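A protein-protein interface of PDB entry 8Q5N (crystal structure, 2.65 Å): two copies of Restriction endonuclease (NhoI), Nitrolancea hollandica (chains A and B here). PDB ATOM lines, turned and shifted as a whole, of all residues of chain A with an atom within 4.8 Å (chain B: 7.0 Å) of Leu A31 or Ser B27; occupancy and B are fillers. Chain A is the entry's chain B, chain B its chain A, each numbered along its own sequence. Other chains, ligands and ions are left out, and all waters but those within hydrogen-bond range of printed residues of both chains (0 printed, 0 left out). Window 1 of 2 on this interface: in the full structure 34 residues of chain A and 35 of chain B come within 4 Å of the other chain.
OG of Ser A27 is in hydrogen-bond range of OH of Tyr B50, at 2.5 Å.
The side-chain amide oxygen (OD1) of Asn B118 is in hydrogen-bond range of the guanidinium group (NE) of Arg A32.
OH of Tyr B50 is in hydrogen-bond range of N of Arg A28 (3.1 Å).
The backbone carbonyl oxygen (O) of Asn B118 lies within hydrogen-bond range of the guanidinium group (NE) of Arg A28 (3.1 Å).
The backbone carbonyl oxygen (O) of Leu A34 is in hydrogen-bond range of the backbone NH (N) of Ile A40.
The backbone carbonyl oxygen (O) of Val B26 lies within hydrogen-bond range of the side-chain hydroxyl (OG) of Ser B30 (3.1 Å).
O of Ser A27 sits at hydrogen-bond distance from OG of Ser A30 (2.7 Å).
OG of Ser B30 is in hydrogen-bond range of O of Ser B27 (2.8 Å).
The backbone carbonyl oxygen (O) of Ile A40 sits close to the side-chain amino group (NZ) of Lys A35 (3.3 Å).
Ser A27 touches Ser B30.
CG of Arg A28 touches CB of Phe B119 (3.7 Å).
Ser A30 touches Leu B23 (CB to O, 3.9 Å).
Leu A31 touches Ser B27.
Leu A31 touches Tyr B50 (CD1 to OH, 3.6 Å).
CB of Leu A31 touches CE1 of Phe B119, at 3.4 Å.
Arg A32 touches Phe B119.
Glu A33 touches Leu B23.
CD1 of Leu A34 touches CD2 of Leu B24 (3.6 Å).
Asp B117 touches Lys A35.
Leu A31 touches just these residues of chain B: Ser B27, Pro B46, Tyr B50 and Phe B119.
Of the printed residues of chain B, Glu A33 touches Leu B23.
Of the printed residues of chain B, Lys A35 touches Asp B117 (3.7 Å).
Ser B27 touches two residues of chain A.
Arg B28 touches none of the printed residues of chain A.
Leu B31 touches none of the printed residues of chain A.
Of the printed residues of chain A, Pro B46 touches Leu A31.
Of the printed residues of chain A, Asp B117 touches Arg A32 (3.6 Å) and Lys A35 (3.7 Å).
The nearest residue of chain B that does not touch Leu A31 is Leu B31 (5.1 Å).
The nearest printed residue of chain A that does not touch Asp B117 is Leu A31 (5.2 Å).
Hydrophobic or aromatic side chains of chain B that line the printed part of chain A: Leu B23, Leu B24, Pro B46, Tyr B50 and Phe B119.
Ser A27 touches Ser B30, and with the chains exchanged Ser A30 touches Ser B27.
Leu A31 touches Ser B27, but with the chains exchanged Ser A27 does not touch Leu B31 (4.1 Å).
Positions printed for both chains: 27, 28, 29, 30, 31, 32 and 33.
Of the 18 pairs that touch across the chains among the printed residues, 2 have their exchanged pair printed and touching as well.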
ATOM      1  N   SER A  27      27.087  24.136 -19.471  1.00  0.00           N
ATOM      2  CA  SER A  27      27.488  25.258 -18.633  1.00  0.00           C
ATOM      3  C   SER A  27      28.838  25.808 -19.066  1.00  0.00           C
ATOM      4  O   SER A  27      29.023  27.028 -19.123  1.00  0.00           O
ATOM      5  CB  SER A  27      27.527  24.832 -17.167  1.00  0.00           C
ATOM      6  OG  SER A  27      28.497  23.822 -16.961  1.00  0.00           O
ATOM      7  N   ARG A  28      29.787  24.927 -19.392  1.00  0.00           N
ATOM      8  CA  ARG A  28      31.121  25.406 -19.731  1.00  0.00           C
ATOM      9  C   ARG A  28      31.112  26.218 -21.018  1.00  0.00           C
ATOM     10  O   ARG A  28      31.877  27.180 -21.146  1.00  0.00           O
ATOM     11  CB  ARG A  28      32.100  24.247 -19.880  1.00  0.00           C
ATOM     12  CG  ARG A  28      33.530  24.729 -19.934  1.00  0.00           C
ATOM     13  CD  ARG A  28      34.469  23.690 -20.489  1.00  0.00           C
ATOM     14  NE  ARG A  28      34.839  24.080 -21.846  1.00  0.00           N
ATOM     15  CZ  ARG A  28      35.564  23.351 -22.682  1.00  0.00           C
ATOM     16  NH1 ARG A  28      35.984  22.137 -22.357  1.00  0.00           N
ATOM     17  NH2 ARG A  28      35.865  23.846 -23.880  1.00  0.00           N
ATOM     18  N   ALA A  29      30.263  25.853 -21.977  1.00  0.00           N
ATOM     19  CA  ALA A  29      30.228  26.570 -23.246  1.00  0.00           C
ATOM     20  C   ALA A  29      29.556  27.932 -23.104  1.00  0.00           C
ATOM     21  O   ALA A  29      30.015  28.916 -23.696  1.00  0.00           O
ATOM     22  CB  ALA A  29      29.519  25.728 -24.307  1.00  0.00           C
ATOM     23  N   SER A  30      28.448  27.995 -22.359  1.00  0.00           N
ATOM     24  CA  SER A  30      27.783  29.272 -22.098  1.00  0.00           C
ATOM     25  C   SER A  30      28.723  30.245 -21.397  1.00  0.00           C
ATOM     26  O   SER A  30      28.804  31.426 -21.761  1.00  0.00           O
ATOM     27  CB  SER A  30      26.528  29.047 -21.257  1.00  0.00           C
ATOM     28  OG  SER A  30      26.842  28.346 -20.065  1.00  0.00           O
ATOM     29  N   LEU A  31      29.414  29.766 -20.361  1.00  0.00           N
ATOM     30  CA  LEU A  31      30.394  30.590 -19.664  1.00  0.00           C
ATOM     31  C   LEU A  31      31.509  31.021 -20.606  1.00  0.00           C
ATOM     32  O   LEU A  31      31.962  32.173 -20.559  1.00  0.00           O
ATOM     33  CB  LEU A  31      30.965  29.816 -18.479  1.00  0.00           C
ATOM     34  CG  LEU A  31      29.969  29.525 -17.360  1.00  0.00           C
ATOM     35  CD1 LEU A  31      30.631  28.699 -16.271  1.00  0.00           C
ATOM     36  CD2 LEU A  31      29.403  30.820 -16.803  1.00  0.00           C
ATOM     37  N   ARG A  32      31.973  30.103 -21.460  1.00  0.00           N
ATOM     38  CA  ARG A  32      32.983  30.445 -22.457  1.00  0.00           C
ATOM     39  C   ARG A  32      32.568  31.663 -23.269  1.00  0.00           C
ATOM     40  O   ARG A  32      33.368  32.579 -23.476  1.00  0.00           O
ATOM     41  CB  ARG A  32      33.212  29.255 -23.390  1.00  0.00           C
ATOM     42  CG  ARG A  32      34.348  29.423 -24.390  1.00  0.00           C
ATOM     43  CD  ARG A  32      34.258  28.343 -25.459  1.00  0.00           C
ATOM     44  NE  ARG A  32      35.348  28.387 -26.426  1.00  0.00           N
ATOM     45  N   GLU A  33      31.306  31.708 -23.698  1.00  0.00           N
ATOM     46  CA  GLU A  33      30.845  32.804 -24.544  1.00  0.00           C
ATOM     47  C   GLU A  33      30.713  34.097 -23.753  1.00  0.00           C
ATOM     48  O   GLU A  33      31.238  35.140 -24.163  1.00  0.00           O
ATOM     49  CB  GLU A  33      29.515  32.441 -25.202  1.00  0.00           C
ATOM     50  CG  GLU A  33      28.998  33.486 -26.181  1.00  0.00           C
ATOM     51  CD  GLU A  33      29.703  33.468 -27.530  1.00  0.00           C
ATOM     52  OE1 GLU A  33      30.933  33.253 -27.583  1.00  0.00           O
ATOM     53  OE2 GLU A  33      29.013  33.676 -28.548  1.00  0.00           O
ATOM     54  N   LEU A  34      29.975  34.055 -22.641  1.00  0.00           N
ATOM     55  CA  LEU A  34      29.876  35.210 -21.756  1.00  0.00           C
ATOM     56  C   LEU A  34      31.241  35.808 -21.463  1.00  0.00           C
ATOM     57  O   LEU A  34      31.393  37.033 -21.390  1.00  0.00           O
ATOM     58  CB  LEU A  34      29.196  34.798 -20.454  1.00  0.00           C
ATOM     59  CG  LEU A  34      27.724  34.448 -20.585  1.00  0.00           C
ATOM     60  CD1 LEU A  34      27.223  33.880 -19.282  1.00  0.00           C
ATOM     61  CD2 LEU A  34      26.957  35.706 -20.954  1.00  0.00           C
ATOM     62  N   LYS A  35      32.247  34.954 -21.291  1.00  0.00           N
ATOM     63  CA  LYS A  35      33.578  35.445 -20.967  1.00  0.00           C
ATOM     64  C   LYS A  35      34.235  36.092 -22.185  1.00  0.00           C
ATOM     65  O   LYS A  35      34.946  37.096 -22.051  1.00  0.00           O
ATOM     66  CB  LYS A  35      34.431  34.305 -20.412  1.00  0.00           C
ATOM     67  CG  LYS A  35      35.886  34.663 -20.232  1.00  0.00           C
ATOM     68  CD  LYS A  35      36.008  35.680 -19.109  1.00  0.00           C
ATOM     69  CE  LYS A  35      37.386  36.298 -19.046  1.00  0.00           C
ATOM     70  NZ  LYS A  35      37.499  37.274 -17.923  1.00  0.00           N
ATOM     71  N   ILE A  40      31.710  38.613 -18.381  1.00  0.00           N
ATOM     72  CA  ILE A  40      32.160  37.969 -17.156  1.00  0.00           C
ATOM     73  C   ILE A  40      33.642  38.260 -16.993  1.00  0.00           C
ATOM     74  O   ILE A  40      34.395  38.258 -17.973  1.00  0.00           O
ATOM     75  CB  ILE A  40      31.890  36.452 -17.219  1.00  0.00           C
ATOM     76  CG1 ILE A  40      30.431  36.141 -16.894  1.00  0.00           C
ATOM     77  CG2 ILE A  40      32.816  35.669 -16.303  1.00  0.00           C
ATOM     78  CD1 ILE A  40      30.124  34.657 -16.921  1.00  0.00           C
ATOM     79  N   GLU B  22      20.196  35.216 -22.127  1.00  0.00           N
ATOM     80  CA  GLU B  22      19.888  33.794 -22.233  1.00  0.00           C
ATOM     81  C   GLU B  22      21.055  32.953 -21.741  1.00  0.00           C
ATOM     82  O   GLU B  22      20.862  31.952 -21.038  1.00  0.00           O
ATOM     83  CB  GLU B  22      19.564  33.441 -23.683  1.00  0.00           C
ATOM     84  CG  GLU B  22      18.222  33.941 -24.179  1.00  0.00           C
ATOM     85  CD  GLU B  22      18.080  33.805 -25.684  1.00  0.00           C
ATOM     86  OE1 GLU B  22      18.783  34.536 -26.414  1.00  0.00           O
ATOM     87  OE2 GLU B  22      17.281  32.958 -26.137  1.00  0.00           O
ATOM     88  N   LEU B  23      22.272  33.355 -22.110  1.00  0.00           N
ATOM     89  CA  LEU B  23      23.476  32.637 -21.715  1.00  0.00           C
ATOM     90  C   LEU B  23      23.571  32.505 -20.199  1.00  0.00           C
ATOM     91  O   LEU B  23      23.916  31.438 -19.679  1.00  0.00           O
ATOM     92  CB  LEU B  23      24.690  33.375 -22.275  1.00  0.00           C
ATOM     93  CG  LEU B  23      24.943  33.226 -23.777  1.00  0.00           C
ATOM     94  CD1 LEU B  23      25.988  34.230 -24.251  1.00  0.00           C
ATOM     95  CD2 LEU B  23      25.343  31.809 -24.143  1.00  0.00           C
ATOM     96  N   LEU B  24      23.286  33.592 -19.477  1.00  0.00           N
ATOM     97  CA  LEU B  24      23.258  33.542 -18.018  1.00  0.00           C
ATOM     98  C   LEU B  24      22.233  32.534 -17.518  1.00  0.00           C
ATOM     99  O   LEU B  24      22.520  31.731 -16.621  1.00  0.00           O
ATOM    100  CB  LEU B  24      22.963  34.933 -17.463  1.00  0.00           C
ATOM    101  CG  LEU B  24      24.089  35.948 -17.649  1.00  0.00           C
ATOM    102  CD1 LEU B  24      23.609  37.335 -17.291  1.00  0.00           C
ATOM    103  CD2 LEU B  24      25.288  35.567 -16.801  1.00  0.00           C
ATOM    104  N   ALA B  25      21.024  32.566 -18.084  1.00  0.00           N
ATOM    105  CA  ALA B  25      19.989  31.624 -17.671  1.00  0.00           C
ATOM    106  C   ALA B  25      20.326  30.205 -18.098  1.00  0.00           C
ATOM    107  O   ALA B  25      19.931  29.246 -17.426  1.00  0.00           O
ATOM    108  CB  ALA B  25      18.635  32.048 -18.241  1.00  0.00           C
ATOM    109  N   VAL B  26      21.050  30.050 -19.206  1.00  0.00           N
ATOM    110  CA  VAL B  26      21.509  28.729 -19.616  1.00  0.00           C
ATOM    111  C   VAL B  26      22.522  28.196 -18.613  1.00  0.00           C
ATOM    112  O   VAL B  26      22.458  27.033 -18.197  1.00  0.00           O
ATOM    113  N   SER B  27      23.468  29.043 -18.204  1.00  0.00           N
ATOM    114  CA  SER B  27      24.483  28.615 -17.247  1.00  0.00           C
ATOM    115  C   SER B  27      23.887  28.383 -15.863  1.00  0.00           C
ATOM    116  O   SER B  27      24.246  27.414 -15.186  1.00  0.00           O
ATOM    117  CB  SER B  27      25.607  29.648 -17.181  1.00  0.00           C
ATOM    118  OG  SER B  27      26.699  29.152 -16.429  1.00  0.00           O
ATOM    119  N   ARG B  28      22.989  29.264 -15.419  1.00  0.00           N
ATOM    120  CA  ARG B  28      22.439  29.129 -14.073  1.00  0.00           C
ATOM    121  C   ARG B  28      21.582  27.879 -13.943  1.00  0.00           C
ATOM    122  O   ARG B  28      21.547  27.255 -12.878  1.00  0.00           O
ATOM    123  CB  ARG B  28      21.633  30.373 -13.693  1.00  0.00           C
ATOM    124  CG  ARG B  28      21.237  30.414 -12.224  1.00  0.00           C
ATOM    125  CD  ARG B  28      20.205  31.491 -11.953  1.00  0.00           C
ATOM    126  NE  ARG B  28      19.424  31.222 -10.751  1.00  0.00           N
ATOM    127  CZ  ARG B  28      19.847  31.433  -9.512  1.00  0.00           C
ATOM    128  NH1 ARG B  28      21.036  31.958  -9.265  1.00  0.00           N
ATOM    129  NH2 ARG B  28      19.046  31.128  -8.493  1.00  0.00           N
ATOM    130  N   ALA B  29      20.882  27.501 -15.012  1.00  0.00           N
ATOM    131  CA  ALA B  29      20.007  26.337 -14.942  1.00  0.00           C
ATOM    132  C   ALA B  29      20.806  25.042 -14.940  1.00  0.00           C
ATOM    133  O   ALA B  29      20.503  24.119 -14.174  1.00  0.00           O
ATOM    134  CB  ALA B  29      19.016  26.355 -16.106  1.00  0.00           C
ATOM    135  N   SER B  30      21.819  24.948 -15.803  1.00  0.00           N
ATOM    136  CA  SER B  30      22.684  23.773 -15.817  1.00  0.00           C
ATOM    137  C   SER B  30      23.367  23.581 -14.471  1.00  0.00           C
ATOM    138  O   SER B  30      23.390  22.472 -13.923  1.00  0.00           O
ATOM    139  CB  SER B  30      23.718  23.904 -16.935  1.00  0.00           C
ATOM    140  OG  SER B  30      24.430  25.123 -16.820  1.00  0.00           O
ATOM    141  N   LEU B  31      23.940  24.656 -13.927  1.00  0.00           N
ATOM    142  CA  LEU B  31      24.577  24.583 -12.618  1.00  0.00           C
ATOM    143  C   LEU B  31      23.576  24.202 -11.534  1.00  0.00           C
ATOM    144  O   LEU B  31      23.889  23.400 -10.647  1.00  0.00           O
ATOM    145  CB  LEU B  31      25.250  25.918 -12.292  1.00  0.00           C
ATOM    146  CG  LEU B  31      26.451  26.282 -13.167  1.00  0.00           C
ATOM    147  CD1 LEU B  31      26.997  27.647 -12.797  1.00  0.00           C
ATOM    148  CD2 LEU B  31      27.542  25.226 -13.058  1.00  0.00           C
ATOM    149  N   ARG B  32      22.370  24.779 -11.585  1.00  0.00           N
ATOM    150  CA  ARG B  32      21.326  24.434 -10.623  1.00  0.00           C
ATOM    151  C   ARG B  32      21.078  22.932 -10.582  1.00  0.00           C
ATOM    152  O   ARG B  32      20.916  22.352  -9.502  1.00  0.00           O
ATOM    153  CB  ARG B  32      20.038  25.191 -10.956  1.00  0.00           C
ATOM    154  N   GLU B  33      21.030  22.287 -11.750  1.00  0.00           N
ATOM    155  CA  GLU B  33      20.770  20.851 -11.794  1.00  0.00           C
ATOM    156  C   GLU B  33      21.987  20.062 -11.327  1.00  0.00           C
ATOM    157  O   GLU B  33      21.868  19.144 -10.509  1.00  0.00           O
ATOM    158  CB  GLU B  33      20.338  20.421 -13.195  1.00  0.00           C
ATOM    159  CG  GLU B  33      19.920  18.954 -13.250  1.00  0.00           C
ATOM    160  CD  GLU B  33      18.958  18.641 -14.382  1.00  0.00           C
ATOM    161  OE1 GLU B  33      18.967  19.367 -15.396  1.00  0.00           O
ATOM    162  OE2 GLU B  33      18.188  17.664 -14.252  1.00  0.00           O
ATOM    163  N   GLY B  43      25.758  27.062  -6.811  1.00  0.00           N
ATOM    164  CA  GLY B  43      25.521  27.495  -8.167  1.00  0.00           C
ATOM    165  C   GLY B  43      26.012  28.902  -8.379  1.00  0.00           C
ATOM    166  O   GLY B  43      25.938  29.423  -9.496  1.00  0.00           O
ATOM    167  N   PRO B  46      30.682  29.773 -10.444  1.00  0.00           N
ATOM    168  CA  PRO B  46      31.056  28.735 -11.426  1.00  0.00           C
ATOM    169  C   PRO B  46      32.522  28.334 -11.437  1.00  0.00           C
ATOM    170  O   PRO B  46      32.814  27.134 -11.403  1.00  0.00           O
ATOM    171  CB  PRO B  46      30.629  29.373 -12.754  1.00  0.00           C
ATOM    172  CG  PRO B  46      29.509  30.274 -12.381  1.00  0.00           C
ATOM    173  CD  PRO B  46      29.885  30.849 -11.054  1.00  0.00           C
ATOM    174  N   ALA B  47      33.455  29.283 -11.506  1.00  0.00           N
ATOM    175  CA  ALA B  47      34.862  28.901 -11.579  1.00  0.00           C
ATOM    176  C   ALA B  47      35.288  28.108 -10.346  1.00  0.00           C
ATOM    177  O   ALA B  47      36.022  27.119 -10.459  1.00  0.00           O
ATOM    178  CB  ALA B  47      35.740  30.138 -11.746  1.00  0.00           C
ATOM    179  N   TYR B  50      33.747  24.537 -10.497  1.00  0.00           N
ATOM    180  CA  TYR B  50      34.471  23.688 -11.437  1.00  0.00           C
ATOM    181  C   TYR B  50      35.770  23.180 -10.829  1.00  0.00           C
ATOM    182  O   TYR B  50      36.049  21.977 -10.850  1.00  0.00           O
ATOM    183  CB  TYR B  50      34.780  24.460 -12.723  1.00  0.00           C
ATOM    184  CG  TYR B  50      33.630  24.630 -13.685  1.00  0.00           C
ATOM    185  CD1 TYR B  50      32.328  24.311 -13.321  1.00  0.00           C
ATOM    186  CD2 TYR B  50      33.852  25.106 -14.969  1.00  0.00           C
ATOM    187  CE1 TYR B  50      31.278  24.472 -14.212  1.00  0.00           C
ATOM    188  CE2 TYR B  50      32.815  25.265 -15.866  1.00  0.00           C
ATOM    189  CZ  TYR B  50      31.531  24.947 -15.483  1.00  0.00           C
ATOM    190  OH  TYR B  50      30.500  25.110 -16.380  1.00  0.00           O
ATOM    191  N   ASP B 117      40.206  31.436 -21.180  1.00  0.00           N
ATOM    192  CA  ASP B 117      38.949  31.893 -21.768  1.00  0.00           C
ATOM    193  C   ASP B 117      37.979  30.764 -22.071  1.00  0.00           C
ATOM    194  O   ASP B 117      36.781  31.021 -22.230  1.00  0.00           O
ATOM    195  CB  ASP B 117      39.211  32.617 -23.084  1.00  0.00           C
ATOM    196  CG  ASP B 117      39.691  34.010 -22.884  1.00  0.00           C
ATOM    197  OD1 ASP B 117      39.111  34.696 -22.019  1.00  0.00           O
ATOM    198  OD2 ASP B 117      40.624  34.424 -23.603  1.00  0.00           O
ATOM    199  N   ASN B 118      38.471  29.541 -22.216  1.00  0.00           N
ATOM    200  CA  ASN B 118      37.634  28.382 -22.482  1.00  0.00           C
ATOM    201  C   ASN B 118      37.121  27.704 -21.225  1.00  0.00           C
ATOM    202  O   ASN B 118      36.403  26.707 -21.339  1.00  0.00           O
ATOM    203  CB  ASN B 118      38.411  27.357 -23.305  1.00  0.00           C
ATOM    204  CG  ASN B 118      38.587  27.777 -24.738  1.00  0.00           C
ATOM    205  OD1 ASN B 118      38.380  28.935 -25.085  1.00  0.00           O
ATOM    206  ND2 ASN B 118      38.966  26.830 -25.587  1.00  0.00           N
ATOM    207  N   PHE B 119      37.504  28.189 -20.046  1.00  0.00           N
ATOM    208  CA  PHE B 119      37.238  27.491 -18.788  1.00  0.00           C
ATOM    209  C   PHE B 119      37.906  26.123 -18.781  1.00  0.00           C
ATOM    210  O   PHE B 119      37.363  25.153 -18.254  1.00  0.00           O
ATOM    211  CB  PHE B 119      35.740  27.362 -18.499  1.00  0.00           C
ATOM    212  CG  PHE B 119      35.123  28.606 -17.933  1.00  0.00           C
ATOM    213  CD1 PHE B 119      34.826  29.679 -18.752  1.00  0.00           C
ATOM    214  CD2 PHE B 119      34.823  28.693 -16.586  1.00  0.00           C
ATOM    215  CE1 PHE B 119      34.254  30.823 -18.234  1.00  0.00           C
ATOM    216  CE2 PHE B 119      34.248  29.831 -16.063  1.00  0.00           C
ATOM    217  CZ  PHE B 119      33.961  30.901 -16.888  1.00  0.00           C
